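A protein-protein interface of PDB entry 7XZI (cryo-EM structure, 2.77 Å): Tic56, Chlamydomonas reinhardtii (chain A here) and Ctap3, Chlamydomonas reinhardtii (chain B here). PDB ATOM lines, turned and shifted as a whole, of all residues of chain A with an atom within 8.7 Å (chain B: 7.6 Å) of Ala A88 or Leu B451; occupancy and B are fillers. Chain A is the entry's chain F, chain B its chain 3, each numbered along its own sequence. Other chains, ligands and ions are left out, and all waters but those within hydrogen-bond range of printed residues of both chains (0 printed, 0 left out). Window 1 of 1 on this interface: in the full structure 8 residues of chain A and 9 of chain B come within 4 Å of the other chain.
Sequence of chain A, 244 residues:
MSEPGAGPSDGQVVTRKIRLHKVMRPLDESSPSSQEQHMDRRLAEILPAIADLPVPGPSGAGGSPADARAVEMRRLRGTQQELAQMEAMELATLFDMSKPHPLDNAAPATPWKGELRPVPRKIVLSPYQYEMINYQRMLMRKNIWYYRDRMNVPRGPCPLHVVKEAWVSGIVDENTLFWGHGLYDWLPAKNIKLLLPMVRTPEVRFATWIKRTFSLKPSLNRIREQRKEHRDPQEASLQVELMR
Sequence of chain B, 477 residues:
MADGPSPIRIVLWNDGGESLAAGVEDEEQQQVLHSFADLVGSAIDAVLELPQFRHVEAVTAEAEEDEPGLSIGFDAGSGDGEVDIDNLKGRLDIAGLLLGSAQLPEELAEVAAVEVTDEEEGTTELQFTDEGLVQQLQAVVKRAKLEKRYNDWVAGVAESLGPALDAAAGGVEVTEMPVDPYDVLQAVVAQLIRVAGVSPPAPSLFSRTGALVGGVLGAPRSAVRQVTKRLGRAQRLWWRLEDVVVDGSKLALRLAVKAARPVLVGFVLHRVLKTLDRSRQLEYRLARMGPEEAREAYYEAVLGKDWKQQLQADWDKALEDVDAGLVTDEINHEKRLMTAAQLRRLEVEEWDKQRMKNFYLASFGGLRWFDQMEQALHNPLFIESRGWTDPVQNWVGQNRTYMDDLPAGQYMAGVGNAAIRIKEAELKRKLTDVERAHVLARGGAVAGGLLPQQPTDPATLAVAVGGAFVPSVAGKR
Of the printed residues of chain B, Gln A81 touches Val B446.
Of the printed residues of chain A, Gly B448 touches Gln A85.
Leu B451 touches just one residue of chain A: Ala A88.
No residue of chain A comes within 4 Å of Pro B452.
The nearest printed residue of chain A that does not touch Ala B447 is Ala A88 (4.7 Å).
Hydrophobic or aromatic side chains of chain A within 4 Å of the printed part of chain B: Ala A84, Ala A88 and Met A89.
Hydrophobic or aromatic side chains of chain B within 4 Å of the printed part of chain A: Leu B450, Leu B451 and Ala B459.
Among the printed residues, 11 pairs touch across the chains.
Among the printed residues, no Asp or Glu carboxylate lies within 4 Å of a Lys or Arg side-chain nitrogen of the other chain.
CG of Gln A81 touches O of Val B446, 3.6 Å away.
O of Val B446 touches CB of Ala A84, 3.6 Å away.
CG of Gln A85 touches O of Ala B447 (3.5 Å).
NE2 of Gln A85 touches CA of Gly B448, at 3.8 Å.
Leu B450 touches Gln A85 (CD1 to O, 3.9 Å).
Leu B450 touches Ala A88 (CB to CB, 3.8 Å).
Leu B451 touches Ala A88 (CD2 to CB, 3.97 Å).
Met A89 touches Leu B450 (CG to CD1, 3.9 Å).
Leu A91 touches Ala B459 (O to CB, 3.8 Å).
Ala A92 touches Ala B459.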
ATOM      1  N   GLN A  81       0.440   7.700 -13.881  1.00  0.00           N
ATOM      2  CA  GLN A  81       0.087   6.285 -13.929  1.00  0.00           C
ATOM      3  C   GLN A  81      -1.423   6.089 -13.857  1.00  0.00           C
ATOM      4  O   GLN A  81      -1.983   5.252 -14.576  1.00  0.00           O
ATOM      5  CB  GLN A  81       0.789   5.540 -12.796  1.00  0.00           C
ATOM      6  CG  GLN A  81       0.680   4.030 -12.875  1.00  0.00           C
ATOM      7  CD  GLN A  81       1.707   3.335 -12.006  1.00  0.00           C
ATOM      8  OE1 GLN A  81       2.775   3.882 -11.731  1.00  0.00           O
ATOM      9  NE2 GLN A  81       1.390   2.124 -11.565  1.00  0.00           N
ATOM     10  N   GLU A  82      -2.097   6.851 -12.993  1.00  0.00           N
ATOM     11  CA  GLU A  82      -3.552   6.769 -12.911  1.00  0.00           C
ATOM     12  C   GLU A  82      -4.199   7.177 -14.228  1.00  0.00           C
ATOM     13  O   GLU A  82      -5.144   6.528 -14.693  1.00  0.00           O
ATOM     14  CB  GLU A  82      -4.063   7.647 -11.770  1.00  0.00           C
ATOM     15  CG  GLU A  82      -5.577   7.699 -11.656  1.00  0.00           C
ATOM     16  CD  GLU A  82      -6.055   8.800 -10.732  1.00  0.00           C
ATOM     17  OE1 GLU A  82      -5.215   9.608 -10.281  1.00  0.00           O
ATOM     18  OE2 GLU A  82      -7.272   8.861 -10.458  1.00  0.00           O
ATOM     19  N   LEU A  83      -3.700   8.250 -14.844  1.00  0.00           N
ATOM     20  CA  LEU A  83      -4.241   8.689 -16.126  1.00  0.00           C
ATOM     21  C   LEU A  83      -4.020   7.637 -17.205  1.00  0.00           C
ATOM     22  O   LEU A  83      -4.905   7.387 -18.030  1.00  0.00           O
ATOM     23  CB  LEU A  83      -3.610  10.021 -16.532  1.00  0.00           C
ATOM     24  CG  LEU A  83      -4.116  10.659 -17.827  1.00  0.00           C
ATOM     25  CD1 LEU A  83      -5.612  10.915 -17.748  1.00  0.00           C
ATOM     26  CD2 LEU A  83      -3.364  11.948 -18.126  1.00  0.00           C
ATOM     27  N   ALA A  84      -2.842   7.009 -17.215  1.00  0.00           N
ATOM     28  CA  ALA A  84      -2.563   5.963 -18.194  1.00  0.00           C
ATOM     29  C   ALA A  84      -3.489   4.768 -18.004  1.00  0.00           C
ATOM     30  O   ALA A  84      -3.999   4.201 -18.977  1.00  0.00           O
ATOM     31  CB  ALA A  84      -1.098   5.535 -18.101  1.00  0.00           C
ATOM     32  N   GLN A  85      -3.713   4.363 -16.752  1.00  0.00           N
ATOM     33  CA  GLN A  85      -4.619   3.247 -16.490  1.00  0.00           C
ATOM     34  C   GLN A  85      -6.047   3.588 -16.901  1.00  0.00           C
ATOM     35  O   GLN A  85      -6.754   2.749 -17.472  1.00  0.00           O
ATOM     36  CB  GLN A  85      -4.562   2.852 -15.014  1.00  0.00           C
ATOM     37  CG  GLN A  85      -3.223   2.284 -14.575  1.00  0.00           C
ATOM     38  CD  GLN A  85      -3.227   1.832 -13.127  1.00  0.00           C
ATOM     39  OE1 GLN A  85      -4.284   1.697 -12.510  1.00  0.00           O
ATOM     40  NE2 GLN A  85      -2.042   1.596 -12.576  1.00  0.00           N
ATOM     41  N   MET A  86      -6.489   4.816 -16.619  1.00  0.00           N
ATOM     42  CA  MET A  86      -7.825   5.235 -17.031  1.00  0.00           C
ATOM     43  C   MET A  86      -7.954   5.251 -18.549  1.00  0.00           C
ATOM     44  O   MET A  86      -8.990   4.853 -19.095  1.00  0.00           O
ATOM     45  CB  MET A  86      -8.150   6.608 -16.447  1.00  0.00           C
ATOM     46  CG  MET A  86      -8.298   6.620 -14.934  1.00  0.00           C
ATOM     47  SD  MET A  86      -9.659   5.584 -14.368  1.00  0.00           S
ATOM     48  CE  MET A  86     -11.035   6.350 -15.219  1.00  0.00           C
ATOM     49  N   GLU A  87      -6.915   5.714 -19.248  1.00  0.00           N
ATOM     50  CA  GLU A  87      -6.950   5.724 -20.707  1.00  0.00           C
ATOM     51  C   GLU A  87      -6.964   4.307 -21.270  1.00  0.00           C
ATOM     52  O   GLU A  87      -7.637   4.042 -22.271  1.00  0.00           O
ATOM     53  CB  GLU A  87      -5.766   6.518 -21.260  1.00  0.00           C
ATOM     54  CG  GLU A  87      -5.870   8.018 -21.018  1.00  0.00           C
ATOM     55  CD  GLU A  87      -4.801   8.812 -21.746  1.00  0.00           C
ATOM     56  OE1 GLU A  87      -3.887   8.192 -22.328  1.00  0.00           O
ATOM     57  OE2 GLU A  87      -4.879  10.059 -21.739  1.00  0.00           O
ATOM     58  N   ALA A  88      -6.229   3.385 -20.645  1.00  0.00           N
ATOM     59  CA  ALA A  88      -6.285   1.989 -21.069  1.00  0.00           C
ATOM     60  C   ALA A  88      -7.677   1.405 -20.855  1.00  0.00           C
ATOM     61  O   ALA A  88      -8.194   0.675 -21.709  1.00  0.00           O
ATOM     62  CB  ALA A  88      -5.234   1.170 -20.322  1.00  0.00           C
ATOM     63  N   MET A  89      -8.300   1.720 -19.717  1.00  0.00           N
ATOM     64  CA  MET A  89      -9.661   1.257 -19.463  1.00  0.00           C
ATOM     65  C   MET A  89     -10.639   1.822 -20.486  1.00  0.00           C
ATOM     66  O   MET A  89     -11.545   1.119 -20.948  1.00  0.00           O
ATOM     67  CB  MET A  89     -10.086   1.638 -18.046  1.00  0.00           C
ATOM     68  CG  MET A  89      -9.354   0.882 -16.953  1.00  0.00           C
ATOM     69  SD  MET A  89      -9.693   1.558 -15.318  1.00  0.00           S
ATOM     70  CE  MET A  89     -11.484   1.599 -15.328  1.00  0.00           C
ATOM     71  N   GLU A  90     -10.479   3.099 -20.842  1.00  0.00           N
ATOM     72  CA  GLU A  90     -11.330   3.701 -21.866  1.00  0.00           C
ATOM     73  C   GLU A  90     -11.107   3.045 -23.224  1.00  0.00           C
ATOM     74  O   GLU A  90     -12.063   2.801 -23.969  1.00  0.00           O
ATOM     75  CB  GLU A  90     -11.068   5.205 -21.941  1.00  0.00           C
ATOM     76  CG  GLU A  90     -11.921   5.942 -22.957  1.00  0.00           C
ATOM     77  CD  GLU A  90     -11.675   7.438 -22.940  1.00  0.00           C
ATOM     78  OE1 GLU A  90     -10.807   7.890 -22.164  1.00  0.00           O
ATOM     79  OE2 GLU A  90     -12.350   8.162 -23.700  1.00  0.00           O
ATOM     80  N   LEU A  91      -9.848   2.758 -23.565  1.00  0.00           N
ATOM     81  CA  LEU A  91      -9.546   2.044 -24.801  1.00  0.00           C
ATOM     82  C   LEU A  91     -10.192   0.666 -24.810  1.00  0.00           C
ATOM     83  O   LEU A  91     -10.596   0.166 -25.866  1.00  0.00           O
ATOM     84  CB  LEU A  91      -8.033   1.920 -24.982  1.00  0.00           C
ATOM     85  CG  LEU A  91      -7.308   3.046 -25.717  1.00  0.00           C
ATOM     86  CD1 LEU A  91      -5.815   2.767 -25.778  1.00  0.00           C
ATOM     87  CD2 LEU A  91      -7.884   3.203 -27.112  1.00  0.00           C
ATOM     88  N   ALA A  92     -10.279   0.030 -23.640  1.00  0.00           N
ATOM     89  CA  ALA A  92     -10.859  -1.306 -23.560  1.00  0.00           C
ATOM     90  C   ALA A  92     -12.310  -1.317 -24.027  1.00  0.00           C
ATOM     91  O   ALA A  92     -12.740  -2.252 -24.711  1.00  0.00           O
ATOM     92  CB  ALA A  92     -10.751  -1.837 -22.130  1.00  0.00           C
ATOM     93  N   THR A  93     -13.081  -0.293 -23.669  1.00  0.00           N
ATOM     94  CA  THR A  93     -14.504  -0.251 -23.977  1.00  0.00           C
ATOM     95  C   THR A  93     -14.889   0.873 -24.932  1.00  0.00           C
ATOM     96  O   THR A  93     -16.059   1.260 -24.965  1.00  0.00           O
ATOM     97  CB  THR A  93     -15.316  -0.123 -22.682  1.00  0.00           C
ATOM     98  OG1 THR A  93     -16.708   0.011 -22.998  1.00  0.00           O
ATOM     99  CG2 THR A  93     -14.862   1.086 -21.880  1.00  0.00           C
ATOM    100  N   LEU A  94     -13.941   1.406 -25.706  1.00  0.00           N
ATOM    101  CA  LEU A  94     -14.239   2.556 -26.556  1.00  0.00           C
ATOM    102  C   LEU A  94     -15.200   2.191 -27.682  1.00  0.00           C
ATOM    103  O   LEU A  94     -16.140   2.938 -27.978  1.00  0.00           O
ATOM    104  CB  LEU A  94     -12.946   3.142 -27.125  1.00  0.00           C
ATOM    105  CG  LEU A  94     -13.132   4.375 -28.012  1.00  0.00           C
ATOM    106  CD1 LEU A  94     -14.001   5.409 -27.318  1.00  0.00           C
ATOM    107  CD2 LEU A  94     -11.793   4.974 -28.370  1.00  0.00           C
ATOM    108  N   VAL B 415       1.389  -0.534 -29.967  1.00  0.00           N
ATOM    109  CA  VAL B 415       1.816   0.576 -29.119  1.00  0.00           C
ATOM    110  C   VAL B 415       3.316   0.507 -28.851  1.00  0.00           C
ATOM    111  O   VAL B 415       4.042   1.491 -29.033  1.00  0.00           O
ATOM    112  CB  VAL B 415       1.010   0.584 -27.810  1.00  0.00           C
ATOM    113  CG1 VAL B 415       1.259   1.871 -27.045  1.00  0.00           C
ATOM    114  CG2 VAL B 415      -0.471   0.403 -28.102  1.00  0.00           C
ATOM    115  N   GLY B 416       3.803  -0.655 -28.411  1.00  0.00           N
ATOM    116  CA  GLY B 416       5.208  -0.768 -28.055  1.00  0.00           C
ATOM    117  C   GLY B 416       6.135  -0.807 -29.255  1.00  0.00           C
ATOM    118  O   GLY B 416       7.189  -0.163 -29.256  1.00  0.00           O
ATOM    119  N   GLY B 443       7.380   0.291 -20.105  1.00  0.00           N
ATOM    120  CA  GLY B 443       6.212   0.838 -20.777  1.00  0.00           C
ATOM    121  C   GLY B 443       4.922   0.166 -20.348  1.00  0.00           C
ATOM    122  O   GLY B 443       3.891   0.824 -20.192  1.00  0.00           O
ATOM    123  N   GLY B 444       4.956  -1.154 -20.164  1.00  0.00           N
ATOM    124  CA  GLY B 444       3.785  -1.845 -19.651  1.00  0.00           C
ATOM    125  C   GLY B 444       3.483  -1.487 -18.209  1.00  0.00           C
ATOM    126  O   GLY B 444       2.318  -1.350 -17.825  1.00  0.00           O
ATOM    127  N   VAL B 446       4.204   1.349 -16.593  1.00  0.00           N
ATOM    128  CA  VAL B 446       3.722   2.718 -16.444  1.00  0.00           C
ATOM    129  C   VAL B 446       2.246   2.833 -16.802  1.00  0.00           C
ATOM    130  O   VAL B 446       1.574   3.771 -16.359  1.00  0.00           O
ATOM    131  CB  VAL B 446       4.578   3.689 -17.288  1.00  0.00           C
ATOM    132  CG1 VAL B 446       4.172   3.643 -18.753  1.00  0.00           C
ATOM    133  CG2 VAL B 446       4.476   5.104 -16.739  1.00  0.00           C
ATOM    134  N   ALA B 447       1.718   1.899 -17.590  1.00  0.00           N
ATOM    135  CA  ALA B 447       0.306   1.878 -17.940  1.00  0.00           C
ATOM    136  C   ALA B 447      -0.497   0.923 -17.067  1.00  0.00           C
ATOM    137  O   ALA B 447      -1.701   0.759 -17.289  1.00  0.00           O
ATOM    138  CB  ALA B 447       0.131   1.509 -19.414  1.00  0.00           C
ATOM    139  N   GLY B 448       0.138   0.291 -16.083  1.00  0.00           N
ATOM    140  CA  GLY B 448      -0.545  -0.637 -15.208  1.00  0.00           C
ATOM    141  C   GLY B 448      -0.745  -2.026 -15.768  1.00  0.00           C
ATOM    142  O   GLY B 448      -1.355  -2.865 -15.096  1.00  0.00           O
ATOM    143  N   GLY B 449      -0.254  -2.300 -16.975  1.00  0.00           N
ATOM    144  CA  GLY B 449      -0.429  -3.596 -17.593  1.00  0.00           C
ATOM    145  C   GLY B 449      -1.792  -3.839 -18.199  1.00  0.00           C
ATOM    146  O   GLY B 449      -2.060  -4.960 -18.649  1.00  0.00           O
ATOM    147  N   LEU B 450      -2.664  -2.830 -18.226  1.00  0.00           N
ATOM    148  CA  LEU B 450      -4.005  -2.999 -18.772  1.00  0.00           C
ATOM    149  C   LEU B 450      -4.044  -2.898 -20.292  1.00  0.00           C
ATOM    150  O   LEU B 450      -5.079  -3.208 -20.889  1.00  0.00           O
ATOM    151  CB  LEU B 450      -4.951  -1.963 -18.162  1.00  0.00           C
ATOM    152  CG  LEU B 450      -5.076  -1.981 -16.638  1.00  0.00           C
ATOM    153  CD1 LEU B 450      -5.983  -0.859 -16.163  1.00  0.00           C
ATOM    154  CD2 LEU B 450      -5.590  -3.326 -16.156  1.00  0.00           C
ATOM    155  N   LEU B 451      -2.957  -2.467 -20.923  1.00  0.00           N
ATOM    156  CA  LEU B 451      -2.942  -2.350 -22.373  1.00  0.00           C
ATOM    157  C   LEU B 451      -3.021  -3.736 -23.011  1.00  0.00           C
ATOM    158  O   LEU B 451      -2.491  -4.706 -22.459  1.00  0.00           O
ATOM    159  CB  LEU B 451      -1.680  -1.625 -22.843  1.00  0.00           C
ATOM    160  CG  LEU B 451      -1.667  -0.108 -22.650  1.00  0.00           C
ATOM    161  CD1 LEU B 451      -0.338   0.481 -23.092  1.00  0.00           C
ATOM    162  CD2 LEU B 451      -2.818   0.528 -23.412  1.00  0.00           C
ATOM    163  N   PRO B 452      -3.680  -3.865 -24.162  1.00  0.00           N
ATOM    164  CA  PRO B 452      -3.781  -5.179 -24.811  1.00  0.00           C
ATOM    165  C   PRO B 452      -2.415  -5.698 -25.236  1.00  0.00           C
ATOM    166  O   PRO B 452      -1.554  -4.941 -25.688  1.00  0.00           O
ATOM    167  CB  PRO B 452      -4.686  -4.906 -26.018  1.00  0.00           C
ATOM    168  CG  PRO B 452      -4.514  -3.450 -26.292  1.00  0.00           C
ATOM    169  CD  PRO B 452      -4.336  -2.808 -24.949  1.00  0.00           C
ATOM    170  N   GLN B 453      -2.224  -7.009 -25.086  1.00  0.00           N
ATOM    171  CA  GLN B 453      -0.989  -7.663 -25.490  1.00  0.00           C
ATOM    172  C   GLN B 453      -1.204  -8.967 -26.240  1.00  0.00           C
ATOM    173  O   GLN B 453      -0.234  -9.511 -26.780  1.00  0.00           O
ATOM    174  CB  GLN B 453      -0.099  -7.932 -24.267  1.00  0.00           C
ATOM    175  CG  GLN B 453      -0.771  -8.755 -23.183  1.00  0.00           C
ATOM    176  CD  GLN B 453       0.062  -8.840 -21.921  1.00  0.00           C
ATOM    177  OE1 GLN B 453       1.043  -8.116 -21.760  1.00  0.00           O
ATOM    178  NE2 GLN B 453      -0.326  -9.730 -21.015  1.00  0.00           N
ATOM    179  N   GLN B 454      -2.423  -9.483 -26.294  1.00  0.00           N
ATOM    180  CA  GLN B 454      -2.743 -10.728 -26.972  1.00  0.00           C
ATOM    181  C   GLN B 454      -3.984 -10.511 -27.825  1.00  0.00           C
ATOM    182  O   GLN B 454      -4.775  -9.599 -27.559  1.00  0.00           O
ATOM    183  CB  GLN B 454      -2.968 -11.869 -25.969  1.00  0.00           C
ATOM    184  CG  GLN B 454      -3.947 -11.544 -24.856  1.00  0.00           C
ATOM    185  CD  GLN B 454      -4.039 -12.648 -23.822  1.00  0.00           C
ATOM    186  OE1 GLN B 454      -3.379 -13.680 -23.938  1.00  0.00           O
ATOM    187  NE2 GLN B 454      -4.860 -12.434 -22.801  1.00  0.00           N
ATOM    188  N   ASP B 457      -7.487  -9.954 -26.279  1.00  0.00           N
ATOM    189  CA  ASP B 457      -7.760  -8.763 -25.489  1.00  0.00           C
ATOM    190  C   ASP B 457      -8.777  -7.878 -26.207  1.00  0.00           C
ATOM    191  O   ASP B 457      -8.713  -7.724 -27.431  1.00  0.00           O
ATOM    192  CB  ASP B 457      -6.470  -7.982 -25.230  1.00  0.00           C
ATOM    193  CG  ASP B 457      -5.611  -8.616 -24.154  1.00  0.00           C
ATOM    194  OD1 ASP B 457      -6.104  -9.526 -23.457  1.00  0.00           O
ATOM    195  OD2 ASP B 457      -4.440  -8.210 -24.003  1.00  0.00           O
ATOM    196  N   ALA B 459      -9.165  -4.719 -26.413  1.00  0.00           N
ATOM    197  CA  ALA B 459      -8.720  -3.396 -26.828  1.00  0.00           C
ATOM    198  C   ALA B 459      -7.785  -3.432 -28.034  1.00  0.00           C
ATOM    199  O   ALA B 459      -7.198  -2.402 -28.384  1.00  0.00           O
ATOM    200  CB  ALA B 459      -8.043  -2.680 -25.659  1.00  0.00           C
ATOM    201  N   THR B 460      -7.635  -4.591 -28.679  1.00  0.00           N
ATOM    202  CA  THR B 460      -6.768  -4.672 -29.851  1.00  0.00           C
ATOM    203  C   THR B 460      -7.368  -3.926 -31.037  1.00  0.00           C
ATOM    204  O   THR B 460      -6.646  -3.258 -31.789  1.00  0.00           O
ATOM    205  CB  THR B 460      -6.511  -6.133 -30.218  1.00  0.00           C
ATOM    206  OG1 THR B 460      -7.760  -6.794 -30.458  1.00  0.00           O
ATOM    207  CG2 THR B 460      -5.773  -6.845 -29.096  1.00  0.00           C
ATOM    208  N   VAL B 463      -6.800  -0.102 -30.871  1.00  0.00           N
ATOM    209  CA  VAL B 463      -5.435   0.270 -31.225  1.00  0.00           C
ATOM    210  C   VAL B 463      -5.220   0.141 -32.728  1.00  0.00           C
ATOM    211  O   VAL B 463      -4.588   1.000 -33.357  1.00  0.00           O
ATOM    212  CB  VAL B 463      -4.428  -0.581 -30.430  1.00  0.00           C
ATOM    213  CG1 VAL B 463      -3.005  -0.228 -30.825  1.00  0.00           C
ATOM    214  CG2 VAL B 463      -4.637  -0.380 -28.939  1.00  0.00           C
